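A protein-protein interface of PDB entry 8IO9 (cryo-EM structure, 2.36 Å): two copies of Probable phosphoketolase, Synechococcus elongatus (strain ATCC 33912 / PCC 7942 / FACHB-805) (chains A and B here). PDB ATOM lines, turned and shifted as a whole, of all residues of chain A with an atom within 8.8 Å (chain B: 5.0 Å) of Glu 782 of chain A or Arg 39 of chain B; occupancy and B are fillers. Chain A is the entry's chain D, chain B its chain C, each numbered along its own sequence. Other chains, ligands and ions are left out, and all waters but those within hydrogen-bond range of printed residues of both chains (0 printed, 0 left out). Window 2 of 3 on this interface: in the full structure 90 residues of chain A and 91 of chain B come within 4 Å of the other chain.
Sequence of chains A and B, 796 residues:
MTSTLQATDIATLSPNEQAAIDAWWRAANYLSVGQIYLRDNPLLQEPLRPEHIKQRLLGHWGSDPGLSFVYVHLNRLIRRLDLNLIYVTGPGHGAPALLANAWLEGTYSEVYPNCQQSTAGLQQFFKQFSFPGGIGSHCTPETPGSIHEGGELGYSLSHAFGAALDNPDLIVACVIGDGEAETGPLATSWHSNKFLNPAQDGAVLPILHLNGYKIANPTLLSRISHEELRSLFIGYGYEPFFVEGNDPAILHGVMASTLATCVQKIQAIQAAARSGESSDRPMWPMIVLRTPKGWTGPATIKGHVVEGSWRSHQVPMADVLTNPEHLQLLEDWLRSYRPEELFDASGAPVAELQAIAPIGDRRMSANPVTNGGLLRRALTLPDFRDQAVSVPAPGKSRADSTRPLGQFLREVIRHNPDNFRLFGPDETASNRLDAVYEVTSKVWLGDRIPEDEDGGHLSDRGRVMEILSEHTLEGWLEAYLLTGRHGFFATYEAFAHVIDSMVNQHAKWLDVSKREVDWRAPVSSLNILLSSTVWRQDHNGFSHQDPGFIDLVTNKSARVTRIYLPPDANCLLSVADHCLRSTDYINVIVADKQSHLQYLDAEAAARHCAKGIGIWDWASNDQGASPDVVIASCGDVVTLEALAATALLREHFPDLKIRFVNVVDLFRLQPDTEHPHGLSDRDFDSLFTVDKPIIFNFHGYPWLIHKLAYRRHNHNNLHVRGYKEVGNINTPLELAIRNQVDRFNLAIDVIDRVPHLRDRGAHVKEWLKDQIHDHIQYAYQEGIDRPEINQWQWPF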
ATOM      1  N   THR A 731      22.469   3.099 -23.451  1.00  0.00           N
ATOM      2  CA  THR A 731      23.541   3.012 -24.415  1.00  0.00           C
ATOM      3  C   THR A 731      23.620   4.325 -25.188  1.00  0.00           C
ATOM      4  O   THR A 731      22.660   5.097 -25.209  1.00  0.00           O
ATOM      5  CB  THR A 731      23.312   1.842 -25.366  1.00  0.00           C
ATOM      6  OG1 THR A 731      22.261   2.163 -26.280  1.00  0.00           O
ATOM      7  CG2 THR A 731      22.927   0.605 -24.591  1.00  0.00           C
ATOM      8  N   ASP A 774      13.898  -1.838 -33.325  1.00  0.00           N
ATOM      9  CA  ASP A 774      14.874  -2.924 -33.325  1.00  0.00           C
ATOM     10  C   ASP A 774      16.071  -2.607 -32.441  1.00  0.00           C
ATOM     11  O   ASP A 774      16.540  -3.471 -31.693  1.00  0.00           O
ATOM     12  CB  ASP A 774      15.337  -3.214 -34.750  1.00  0.00           C
ATOM     13  CG  ASP A 774      14.258  -3.849 -35.591  1.00  0.00           C
ATOM     14  OD1 ASP A 774      13.174  -4.146 -35.048  1.00  0.00           O
ATOM     15  OD2 ASP A 774      14.494  -4.055 -36.800  1.00  0.00           O
ATOM     16  N   HIS A 775      16.585  -1.381 -32.517  1.00  0.00           N
ATOM     17  CA  HIS A 775      17.774  -1.041 -31.747  1.00  0.00           C
ATOM     18  C   HIS A 775      17.476  -0.937 -30.259  1.00  0.00           C
ATOM     19  O   HIS A 775      18.337  -1.261 -29.437  1.00  0.00           O
ATOM     20  CB  HIS A 775      18.384   0.256 -32.270  1.00  0.00           C
ATOM     21  CG  HIS A 775      19.061   0.103 -33.594  1.00  0.00           C
ATOM     22  ND1 HIS A 775      20.245  -0.585 -33.747  1.00  0.00           N
ATOM     23  CD2 HIS A 775      18.720   0.543 -34.828  1.00  0.00           C
ATOM     24  CE1 HIS A 775      20.602  -0.564 -35.018  1.00  0.00           C
ATOM     25  NE2 HIS A 775      19.694   0.115 -35.694  1.00  0.00           N
ATOM     26  N   ILE A 776      16.279  -0.478 -29.893  1.00  0.00           N
ATOM     27  CA  ILE A 776      15.902  -0.464 -28.483  1.00  0.00           C
ATOM     28  C   ILE A 776      15.786  -1.886 -27.949  1.00  0.00           C
ATOM     29  O   ILE A 776      16.252  -2.187 -26.844  1.00  0.00           O
ATOM     30  CB  ILE A 776      14.597   0.326 -28.281  1.00  0.00           C
ATOM     31  CG1 ILE A 776      14.817   1.806 -28.581  1.00  0.00           C
ATOM     32  CG2 ILE A 776      14.099   0.170 -26.858  1.00  0.00           C
ATOM     33  CD1 ILE A 776      15.717   2.494 -27.592  1.00  0.00           C
ATOM     34  N   GLN A 777      15.164  -2.782 -28.720  1.00  0.00           N
ATOM     35  CA  GLN A 777      15.033  -4.168 -28.280  1.00  0.00           C
ATOM     36  C   GLN A 777      16.394  -4.830 -28.134  1.00  0.00           C
ATOM     37  O   GLN A 777      16.630  -5.576 -27.178  1.00  0.00           O
ATOM     38  CB  GLN A 777      14.160  -4.956 -29.255  1.00  0.00           C
ATOM     39  CG  GLN A 777      12.724  -4.474 -29.343  1.00  0.00           C
ATOM     40  CD  GLN A 777      12.069  -4.325 -27.987  1.00  0.00           C
ATOM     41  OE1 GLN A 777      12.185  -5.196 -27.127  1.00  0.00           O
ATOM     42  NE2 GLN A 777      11.378  -3.209 -27.787  1.00  0.00           N
ATOM     43  N   TYR A 778      17.299  -4.580 -29.080  1.00  0.00           N
ATOM     44  CA  TYR A 778      18.654  -5.105 -28.960  1.00  0.00           C
ATOM     45  C   TYR A 778      19.366  -4.508 -27.754  1.00  0.00           C
ATOM     46  O   TYR A 778      20.141  -5.191 -27.080  1.00  0.00           O
ATOM     47  CB  TYR A 778      19.437  -4.829 -30.241  1.00  0.00           C
ATOM     48  CG  TYR A 778      20.775  -5.523 -30.312  1.00  0.00           C
ATOM     49  CD1 TYR A 778      21.911  -4.945 -29.765  1.00  0.00           C
ATOM     50  CD2 TYR A 778      20.906  -6.753 -30.935  1.00  0.00           C
ATOM     51  CE1 TYR A 778      23.132  -5.572 -29.831  1.00  0.00           C
ATOM     52  CE2 TYR A 778      22.124  -7.389 -31.006  1.00  0.00           C
ATOM     53  CZ  TYR A 778      23.233  -6.794 -30.453  1.00  0.00           C
ATOM     54  OH  TYR A 778      24.452  -7.425 -30.521  1.00  0.00           O
ATOM     55  N   ALA A 779      19.124  -3.226 -27.478  1.00  0.00           N
ATOM     56  CA  ALA A 779      19.762  -2.580 -26.338  1.00  0.00           C
ATOM     57  C   ALA A 779      19.318  -3.205 -25.024  1.00  0.00           C
ATOM     58  O   ALA A 779      20.137  -3.422 -24.124  1.00  0.00           O
ATOM     59  CB  ALA A 779      19.456  -1.085 -26.348  1.00  0.00           C
ATOM     60  N   TYR A 780      18.024  -3.494 -24.888  1.00  0.00           N
ATOM     61  CA  TYR A 780      17.536  -4.140 -23.678  1.00  0.00           C
ATOM     62  C   TYR A 780      17.971  -5.592 -23.587  1.00  0.00           C
ATOM     63  O   TYR A 780      17.917  -6.176 -22.500  1.00  0.00           O
ATOM     64  CB  TYR A 780      16.013  -4.052 -23.609  1.00  0.00           C
ATOM     65  CG  TYR A 780      15.506  -2.676 -23.256  1.00  0.00           C
ATOM     66  CD1 TYR A 780      16.297  -1.788 -22.545  1.00  0.00           C
ATOM     67  CD2 TYR A 780      14.238  -2.266 -23.632  1.00  0.00           C
ATOM     68  CE1 TYR A 780      15.843  -0.532 -22.219  1.00  0.00           C
ATOM     69  CE2 TYR A 780      13.774  -1.010 -23.309  1.00  0.00           C
ATOM     70  CZ  TYR A 780      14.581  -0.148 -22.603  1.00  0.00           C
ATOM     71  OH  TYR A 780      14.121   1.106 -22.280  1.00  0.00           O
ATOM     72  N   GLN A 781      18.391  -6.186 -24.698  1.00  0.00           N
ATOM     73  CA  GLN A 781      18.793  -7.585 -24.728  1.00  0.00           C
ATOM     74  C   GLN A 781      20.278  -7.773 -24.452  1.00  0.00           C
ATOM     75  O   GLN A 781      20.658  -8.691 -23.721  1.00  0.00           O
ATOM     76  CB  GLN A 781      18.430  -8.189 -26.083  1.00  0.00           C
ATOM     77  CG  GLN A 781      19.002  -9.563 -26.338  1.00  0.00           C
ATOM     78  CD  GLN A 781      18.740 -10.034 -27.752  1.00  0.00           C
ATOM     79  OE1 GLN A 781      17.953  -9.430 -28.482  1.00  0.00           O
ATOM     80  NE2 GLN A 781      19.401 -11.113 -28.150  1.00  0.00           N
ATOM     81  N   GLU A 782      21.129  -6.917 -25.014  1.00  0.00           N
ATOM     82  CA  GLU A 782      22.573  -7.087 -24.925  1.00  0.00           C
ATOM     83  C   GLU A 782      23.270  -6.038 -24.078  1.00  0.00           C
ATOM     84  O   GLU A 782      24.355  -6.306 -23.561  1.00  0.00           O
ATOM     85  CB  GLU A 782      23.191  -7.076 -26.326  1.00  0.00           C
ATOM     86  CG  GLU A 782      22.494  -7.993 -27.309  1.00  0.00           C
ATOM     87  CD  GLU A 782      22.725  -9.460 -27.010  1.00  0.00           C
ATOM     88  OE1 GLU A 782      23.686  -9.780 -26.282  1.00  0.00           O
ATOM     89  OE2 GLU A 782      21.945 -10.296 -27.510  1.00  0.00           O
ATOM     90  N   GLY A 783      22.689  -4.853 -23.928  1.00  0.00           N
ATOM     91  CA  GLY A 783      23.304  -3.800 -23.153  1.00  0.00           C
ATOM     92  C   GLY A 783      24.193  -2.859 -23.931  1.00  0.00           C
ATOM     93  O   GLY A 783      24.712  -1.901 -23.346  1.00  0.00           O
ATOM     94  N   ILE A 784      24.397  -3.102 -25.226  1.00  0.00           N
ATOM     95  CA  ILE A 784      25.164  -2.216 -26.091  1.00  0.00           C
ATOM     96  C   ILE A 784      24.442  -2.103 -27.427  1.00  0.00           C
ATOM     97  O   ILE A 784      23.463  -2.800 -27.694  1.00  0.00           O
ATOM     98  CB  ILE A 784      26.611  -2.702 -26.318  1.00  0.00           C
ATOM     99  CG1 ILE A 784      26.611  -4.161 -26.771  1.00  0.00           C
ATOM    100  CG2 ILE A 784      27.449  -2.501 -25.071  1.00  0.00           C
ATOM    101  CD1 ILE A 784      27.934  -4.622 -27.317  1.00  0.00           C
ATOM    102  N   ASP A 785      24.946  -1.211 -28.270  1.00  0.00           N
ATOM    103  CA  ASP A 785      24.416  -1.052 -29.611  1.00  0.00           C
ATOM    104  C   ASP A 785      24.993  -2.116 -30.537  1.00  0.00           C
ATOM    105  O   ASP A 785      25.987  -2.777 -30.227  1.00  0.00           O
ATOM    106  CB  ASP A 785      24.736   0.340 -30.149  1.00  0.00           C
ATOM    107  CG  ASP A 785      24.376   1.438 -29.170  1.00  0.00           C
ATOM    108  OD1 ASP A 785      23.328   1.318 -28.505  1.00  0.00           O
ATOM    109  OD2 ASP A 785      25.143   2.418 -29.062  1.00  0.00           O
ATOM    110  N   ARG A 786      24.351  -2.275 -31.688  1.00  0.00           N
ATOM    111  CA  ARG A 786      24.813  -3.241 -32.667  1.00  0.00           C
ATOM    112  C   ARG A 786      26.178  -2.829 -33.214  1.00  0.00           C
ATOM    113  O   ARG A 786      26.531  -1.648 -33.193  1.00  0.00           O
ATOM    114  CB  ARG A 786      23.807  -3.363 -33.806  1.00  0.00           C
ATOM    115  CG  ARG A 786      22.540  -4.089 -33.424  1.00  0.00           C
ATOM    116  CD  ARG A 786      21.585  -4.177 -34.595  1.00  0.00           C
ATOM    117  NE  ARG A 786      20.455  -5.046 -34.302  1.00  0.00           N
ATOM    118  CZ  ARG A 786      20.455  -6.358 -34.494  1.00  0.00           C
ATOM    119  NH1 ARG A 786      21.512  -6.985 -34.982  1.00  0.00           N
ATOM    120  NH2 ARG A 786      19.367  -7.058 -34.190  1.00  0.00           N
ATOM    121  N   PRO A 787      26.977  -3.789 -33.685  1.00  0.00           N
ATOM    122  CA  PRO A 787      28.305  -3.438 -34.209  1.00  0.00           C
ATOM    123  C   PRO A 787      28.266  -2.454 -35.361  1.00  0.00           C
ATOM    124  O   PRO A 787      29.167  -1.614 -35.475  1.00  0.00           O
ATOM    125  CB  PRO A 787      28.874  -4.794 -34.647  1.00  0.00           C
ATOM    126  CG  PRO A 787      28.153  -5.786 -33.818  1.00  0.00           C
ATOM    127  CD  PRO A 787      26.768  -5.245 -33.653  1.00  0.00           C
ATOM    128  N   TYR B  37      29.993  -7.577 -13.426  1.00  0.00           N
ATOM    129  CA  TYR B  37      30.478  -8.363 -14.550  1.00  0.00           C
ATOM    130  C   TYR B  37      29.434  -9.292 -15.147  1.00  0.00           C
ATOM    131  O   TYR B  37      29.186  -9.241 -16.354  1.00  0.00           O
ATOM    132  CB  TYR B  37      31.695  -9.180 -14.115  1.00  0.00           C
ATOM    133  CG  TYR B  37      32.920  -8.348 -13.856  1.00  0.00           C
ATOM    134  CD1 TYR B  37      33.798  -8.045 -14.880  1.00  0.00           C
ATOM    135  CD2 TYR B  37      33.198  -7.862 -12.591  1.00  0.00           C
ATOM    136  CE1 TYR B  37      34.924  -7.292 -14.651  1.00  0.00           C
ATOM    137  CE2 TYR B  37      34.318  -7.105 -12.355  1.00  0.00           C
ATOM    138  CZ  TYR B  37      35.177  -6.825 -13.388  1.00  0.00           C
ATOM    139  OH  TYR B  37      36.298  -6.071 -13.151  1.00  0.00           O
ATOM    140  N   LEU B  38      28.815 -10.144 -14.340  1.00  0.00           N
ATOM    141  CA  LEU B  38      28.007 -11.225 -14.880  1.00  0.00           C
ATOM    142  C   LEU B  38      26.652 -10.731 -15.356  1.00  0.00           C
ATOM    143  O   LEU B  38      26.020  -9.884 -14.719  1.00  0.00           O
ATOM    144  CB  LEU B  38      27.810 -12.318 -13.835  1.00  0.00           C
ATOM    145  CG  LEU B  38      29.087 -12.884 -13.224  1.00  0.00           C
ATOM    146  CD1 LEU B  38      28.763 -14.111 -12.403  1.00  0.00           C
ATOM    147  CD2 LEU B  38      30.102 -13.207 -14.301  1.00  0.00           C
ATOM    148  N   ARG B  39      26.207 -11.274 -16.484  1.00  0.00           N
ATOM    149  CA  ARG B  39      24.835 -11.130 -16.939  1.00  0.00           C
ATOM    150  C   ARG B  39      24.124 -12.470 -17.014  1.00  0.00           C
ATOM    151  O   ARG B  39      22.924 -12.509 -17.305  1.00  0.00           O
ATOM    152  CB  ARG B  39      24.783 -10.452 -18.312  1.00  0.00           C
ATOM    153  CG  ARG B  39      25.368 -11.295 -19.421  1.00  0.00           C
ATOM    154  CD  ARG B  39      25.119 -10.674 -20.772  1.00  0.00           C
ATOM    155  NE  ARG B  39      23.697 -10.469 -21.001  1.00  0.00           N
ATOM    156  CZ  ARG B  39      23.173 -10.071 -22.151  1.00  0.00           C
ATOM    157  NH1 ARG B  39      23.929  -9.833 -23.210  1.00  0.00           N
ATOM    158  NH2 ARG B  39      21.856  -9.911 -22.241  1.00  0.00           N
ATOM    159  N   ASP B  40      24.834 -13.566 -16.767  1.00  0.00           N
ATOM    160  CA  ASP B  40      24.268 -14.903 -16.797  1.00  0.00           C
ATOM    161  C   ASP B  40      25.186 -15.804 -15.989  1.00  0.00           C
ATOM    162  O   ASP B  40      26.332 -15.447 -15.705  1.00  0.00           O
ATOM    163  CB  ASP B  40      24.116 -15.414 -18.232  1.00  0.00           C
ATOM    164  CG  ASP B  40      23.111 -16.536 -18.348  1.00  0.00           C
ATOM    165  OD1 ASP B  40      22.843 -17.208 -17.330  1.00  0.00           O
ATOM    166  OD2 ASP B  40      22.589 -16.748 -19.462  1.00  0.00           O
ATOM    167  N   ASN B  41      24.669 -16.978 -15.624  1.00  0.00           N
ATOM    168  CA  ASN B  41      25.395 -17.947 -14.809  1.00  0.00           C
ATOM    169  C   ASN B  41      25.842 -17.295 -13.506  1.00  0.00           C
ATOM    170  O   ASN B  41      27.037 -17.039 -13.315  1.00  0.00           O
ATOM    171  CB  ASN B  41      26.595 -18.509 -15.575  1.00  0.00           C
ATOM    172  CG  ASN B  41      27.281 -19.636 -14.836  1.00  0.00           C
ATOM    173  OD1 ASN B  41      26.633 -20.449 -14.180  1.00  0.00           O
ATOM    174  ND2 ASN B  41      28.603 -19.686 -14.932  1.00  0.00           N
ATOM    175  N   GLU B  51      29.771 -15.191 -23.059  1.00  0.00           N
ATOM    176  CA  GLU B  51      28.344 -14.910 -23.132  1.00  0.00           C
ATOM    177  C   GLU B  51      27.730 -14.620 -21.769  1.00  0.00           C
ATOM    178  O   GLU B  51      26.577 -14.182 -21.712  1.00  0.00           O
ATOM    179  CB  GLU B  51      27.604 -16.071 -23.799  1.00  0.00           C
ATOM    180  CG  GLU B  51      27.929 -17.444 -23.236  1.00  0.00           C
ATOM    181  CD  GLU B  51      29.121 -18.091 -23.918  1.00  0.00           C
ATOM    182  OE1 GLU B  51      30.028 -17.357 -24.367  1.00  0.00           O
ATOM    183  OE2 GLU B  51      29.152 -19.337 -24.007  1.00  0.00           O
ATOM    184  N   HIS B  52      28.460 -14.856 -20.682  1.00  0.00           N
ATOM    185  CA  HIS B  52      27.973 -14.538 -19.348  1.00  0.00           C
ATOM    186  C   HIS B  52      28.412 -13.165 -18.867  1.00  0.00           C
ATOM    187  O   HIS B  52      27.849 -12.656 -17.892  1.00  0.00           O
ATOM    188  CB  HIS B  52      28.451 -15.594 -18.350  1.00  0.00           C
ATOM    189  CG  HIS B  52      28.077 -16.991 -18.726  1.00  0.00           C
ATOM    190  ND1 HIS B  52      28.846 -18.084 -18.392  1.00  0.00           N
ATOM    191  CD2 HIS B  52      27.011 -17.474 -19.407  1.00  0.00           C
ATOM    192  CE1 HIS B  52      28.271 -19.180 -18.852  1.00  0.00           C
ATOM    193  NE2 HIS B  52      27.156 -18.837 -19.471  1.00  0.00           N
ATOM    194  N   ILE B  53      29.402 -12.565 -19.509  1.00  0.00           N
ATOM    195  CA  ILE B  53      29.927 -11.276 -19.078  1.00  0.00           C
ATOM    196  C   ILE B  53      29.124 -10.158 -19.724  1.00  0.00           C
ATOM    197  O   ILE B  53      28.677 -10.271 -20.870  1.00  0.00           O
ATOM    198  CB  ILE B  53      31.423 -11.167 -19.420  1.00  0.00           C
ATOM    199  CG1 ILE B  53      32.153 -12.421 -18.958  1.00  0.00           C
ATOM    200  CG2 ILE B  53      32.038  -9.954 -18.752  1.00  0.00           C
ATOM    201  CD1 ILE B  53      32.010 -12.677 -17.490  1.00  0.00           C
ATOM    202  N   LYS B  54      28.927  -9.074 -18.977  1.00  0.00           N
ATOM    203  CA  LYS B  54      28.258  -7.903 -19.519  1.00  0.00           C
ATOM    204  C   LYS B  54      29.128  -7.231 -20.572  1.00  0.00           C
ATOM    205  O   LYS B  54      30.352  -7.158 -20.438  1.00  0.00           O
ATOM    206  CB  LYS B  54      27.928  -6.918 -18.402  1.00  0.00           C
ATOM    207  CG  LYS B  54      26.788  -7.365 -17.515  1.00  0.00           C
ATOM    208  CD  LYS B  54      26.543  -6.378 -16.398  1.00  0.00           C
ATOM    209  CE  LYS B  54      25.335  -6.782 -15.587  1.00  0.00           C
ATOM    210  NZ  LYS B  54      25.168  -5.923 -14.392  1.00  0.00           N
ATOM    211  N   GLN B  55      28.482  -6.737 -21.628  1.00  0.00           N
ATOM    212  CA  GLN B  55      29.216  -6.130 -22.732  1.00  0.00           C
ATOM    213  C   GLN B  55      29.928  -4.860 -22.287  1.00  0.00           C
ATOM    214  O   GLN B  55      31.125  -4.683 -22.542  1.00  0.00           O
ATOM    215  CB  GLN B  55      28.263  -5.836 -23.887  1.00  0.00           C
ATOM    216  CG  GLN B  55      27.479  -7.039 -24.364  1.00  0.00           C
ATOM    217  CD  GLN B  55      28.324  -8.004 -25.162  1.00  0.00           C
ATOM    218  OE1 GLN B  55      29.405  -7.656 -25.634  1.00  0.00           O
ATOM    219  NE2 GLN B  55      27.834  -9.226 -25.321  1.00  0.00           N
ATOM    220  N   GLN B 123      19.974 -14.403 -11.240  1.00  0.00           N
ATOM    221  CA  GLN B 123      20.160 -14.101 -12.654  1.00  0.00           C
ATOM    222  C   GLN B 123      19.544 -12.756 -13.006  1.00  0.00           C
ATOM    223  O   GLN B 123      20.134 -11.970 -13.753  1.00  0.00           O
ATOM    224  CB  GLN B 123      19.564 -15.217 -13.512  1.00  0.00           C
ATOM    225  CG  GLN B 123      19.987 -15.180 -14.973  1.00  0.00           C
ATOM    226  CD  GLN B 123      19.129 -14.256 -15.814  1.00  0.00           C
ATOM    227  OE1 GLN B 123      17.932 -14.108 -15.571  1.00  0.00           O
ATOM    228  NE2 GLN B 123      19.739 -13.626 -16.809  1.00  0.00           N
ATOM    229  N   PHE B 126      21.699 -10.013 -11.055  1.00  0.00           N
ATOM    230  CA  PHE B 126      22.985  -9.681 -11.659  1.00  0.00           C
ATOM    231  C   PHE B 126      22.812  -8.951 -12.983  1.00  0.00           C
ATOM    232  O   PHE B 126      23.552  -8.008 -13.280  1.00  0.00           O
ATOM    233  CB  PHE B 126      23.814 -10.945 -11.861  1.00  0.00           C
ATOM    234  CG  PHE B 126      24.602 -11.346 -10.657  1.00  0.00           C
ATOM    235  CD1 PHE B 126      24.866 -10.432  -9.655  1.00  0.00           C
ATOM    236  CD2 PHE B 126      25.082 -12.632 -10.527  1.00  0.00           C
ATOM    237  CE1 PHE B 126      25.590 -10.796  -8.548  1.00  0.00           C
ATOM    238  CE2 PHE B 126      25.808 -13.000  -9.418  1.00  0.00           C
ATOM    239  CZ  PHE B 126      26.063 -12.081  -8.429  1.00  0.00           C
ATOM    240  N   LYS B 127      21.845  -9.375 -13.794  1.00  0.00           N
ATOM    241  CA  LYS B 127      21.689  -8.813 -15.127  1.00  0.00           C
ATOM    242  C   LYS B 127      21.151  -7.391 -15.099  1.00  0.00           C
ATOM    243  O   LYS B 127      21.385  -6.636 -16.047  1.00  0.00           O
ATOM    244  CB  LYS B 127      20.769  -9.707 -15.955  1.00  0.00           C
ATOM    245  CG  LYS B 127      20.789  -9.433 -17.442  1.00  0.00           C
ATOM    246  CD  LYS B 127      19.490  -8.810 -17.904  1.00  0.00           C
ATOM    247  CE  LYS B 127      19.437  -8.730 -19.417  1.00  0.00           C
ATOM    248  NZ  LYS B 127      18.144  -8.175 -19.898  1.00  0.00           N
ATOM    249  N   PHE B 131      22.419  -1.627 -16.440  1.00  0.00           N
ATOM    250  CA  PHE B 131      21.982  -2.237 -17.673  1.00  0.00           C
ATOM    251  C   PHE B 131      20.806  -1.450 -18.231  1.00  0.00           C
ATOM    252  O   PHE B 131      19.984  -0.936 -17.460  1.00  0.00           O
ATOM    253  CB  PHE B 131      21.573  -3.695 -17.439  1.00  0.00           C
ATOM    254  CG  PHE B 131      21.695  -4.559 -18.650  1.00  0.00           C
ATOM    255  CD1 PHE B 131      22.910  -5.120 -18.991  1.00  0.00           C
ATOM    256  CD2 PHE B 131      20.595  -4.817 -19.444  1.00  0.00           C
ATOM    257  CE1 PHE B 131      23.027  -5.916 -20.104  1.00  0.00           C
ATOM    258  CE2 PHE B 131      20.706  -5.613 -20.561  1.00  0.00           C
ATOM    259  CZ  PHE B 131      21.922  -6.165 -20.891  1.00  0.00           C
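O of His 52 of chain B lies within hydrogen-bond range of N of Arg 39 of chain B (2.6 Å).
NE2 of Gln 123 of chain B is in hydrogen-bond range of O of Arg 39 of chain B (3.4 Å).
The side-chain amide nitrogen (NE2) of Gln 781 of chain A is in hydrogen-bond range of the side-chain carboxylate (OE2) of Glu 782 of chain A, 2.7 Å away.
The guanidinium group (NH1) of Arg 39 of chain B lies within salt-bridge range of the side-chain carboxylate (OE1) of Glu 782 of chain A (3.1 Å).
The side-chain amino group (NZ) of Lys 127 of chain B lies within hydrogen-bond range of the backbone carbonyl oxygen (O) of Tyr 780 of chain A, 3.3 Å away.
NH2 of Arg 39 of chain B lies close to O of Gln 781 of chain A (2.3 Å).
Printed residues of chain B within 4 Å of Tyr 780 of chain A: Lys 127 (3.3 Å) and Phe 131 (3.4 Å).
Of the printed residues of chain B, Gln 781 of chain A touches Arg 39 and Phe 131.
Glu 782 of chain A touches just these residues of chain B: Arg 39, Gln 55 and Phe 131.
Printed residues of chain B within 4 Å of Gly 783 of chain A: Phe 131.
Arg 39 of chain B touches two residues of chain A.
Printed residues of chain A within 4 Å of Gln 55 of chain B: Glu 782 and Ile 784.
Gln 123 of chain B touches none of the printed residues of chain A.
Of the printed residues of chain A, Lys 127 of chain B touches Tyr 780 (3.3 Å).
The nearest printed residue of chain B that does not touch Glu 782 of chain A is Lys 54 of chain B (5.7 Å).
The nearest residue of chain A that does not touch Arg 39 of chain B is Gly 783 of chain A (5.2 Å).
The nearest printed residue of chain B that does not touch Gln 781 of chain A is Lys 127 of chain B (4.5 Å).
No position is printed for both chains.
Of the 9 pairs that touch across the chains among the printed residues, none has its exchanged pair printed and touching as well.
Among the printed residues, pairs that only touch across the chains: Tyr 780 of chain A with Phe 131 of chain B, Gln 781 of chain A with Phe 131 of chain B, Glu 782 of chain A with Gln 55 of chain B, Glu 782 of chain A with Phe 131 of chain B, Gly 783 of chain A with Phe 131 of chain B and Ile 784 of chain A with Gln 55 of chain B.
Printed residues of chain B that touch a printed residue of chain A: Arg 39, Gln 55, Lys 127 and Phe 131.
Along chain B the printed residues that touch a printed residue of chain A span positions 39 to 131.
Printed residues of chain A that touch a printed residue of chain B: Tyr 780, Gln 781, Glu 782, Gly 783 and Ile 784.
Among the printed residues, 9 pairs touch across the chains.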
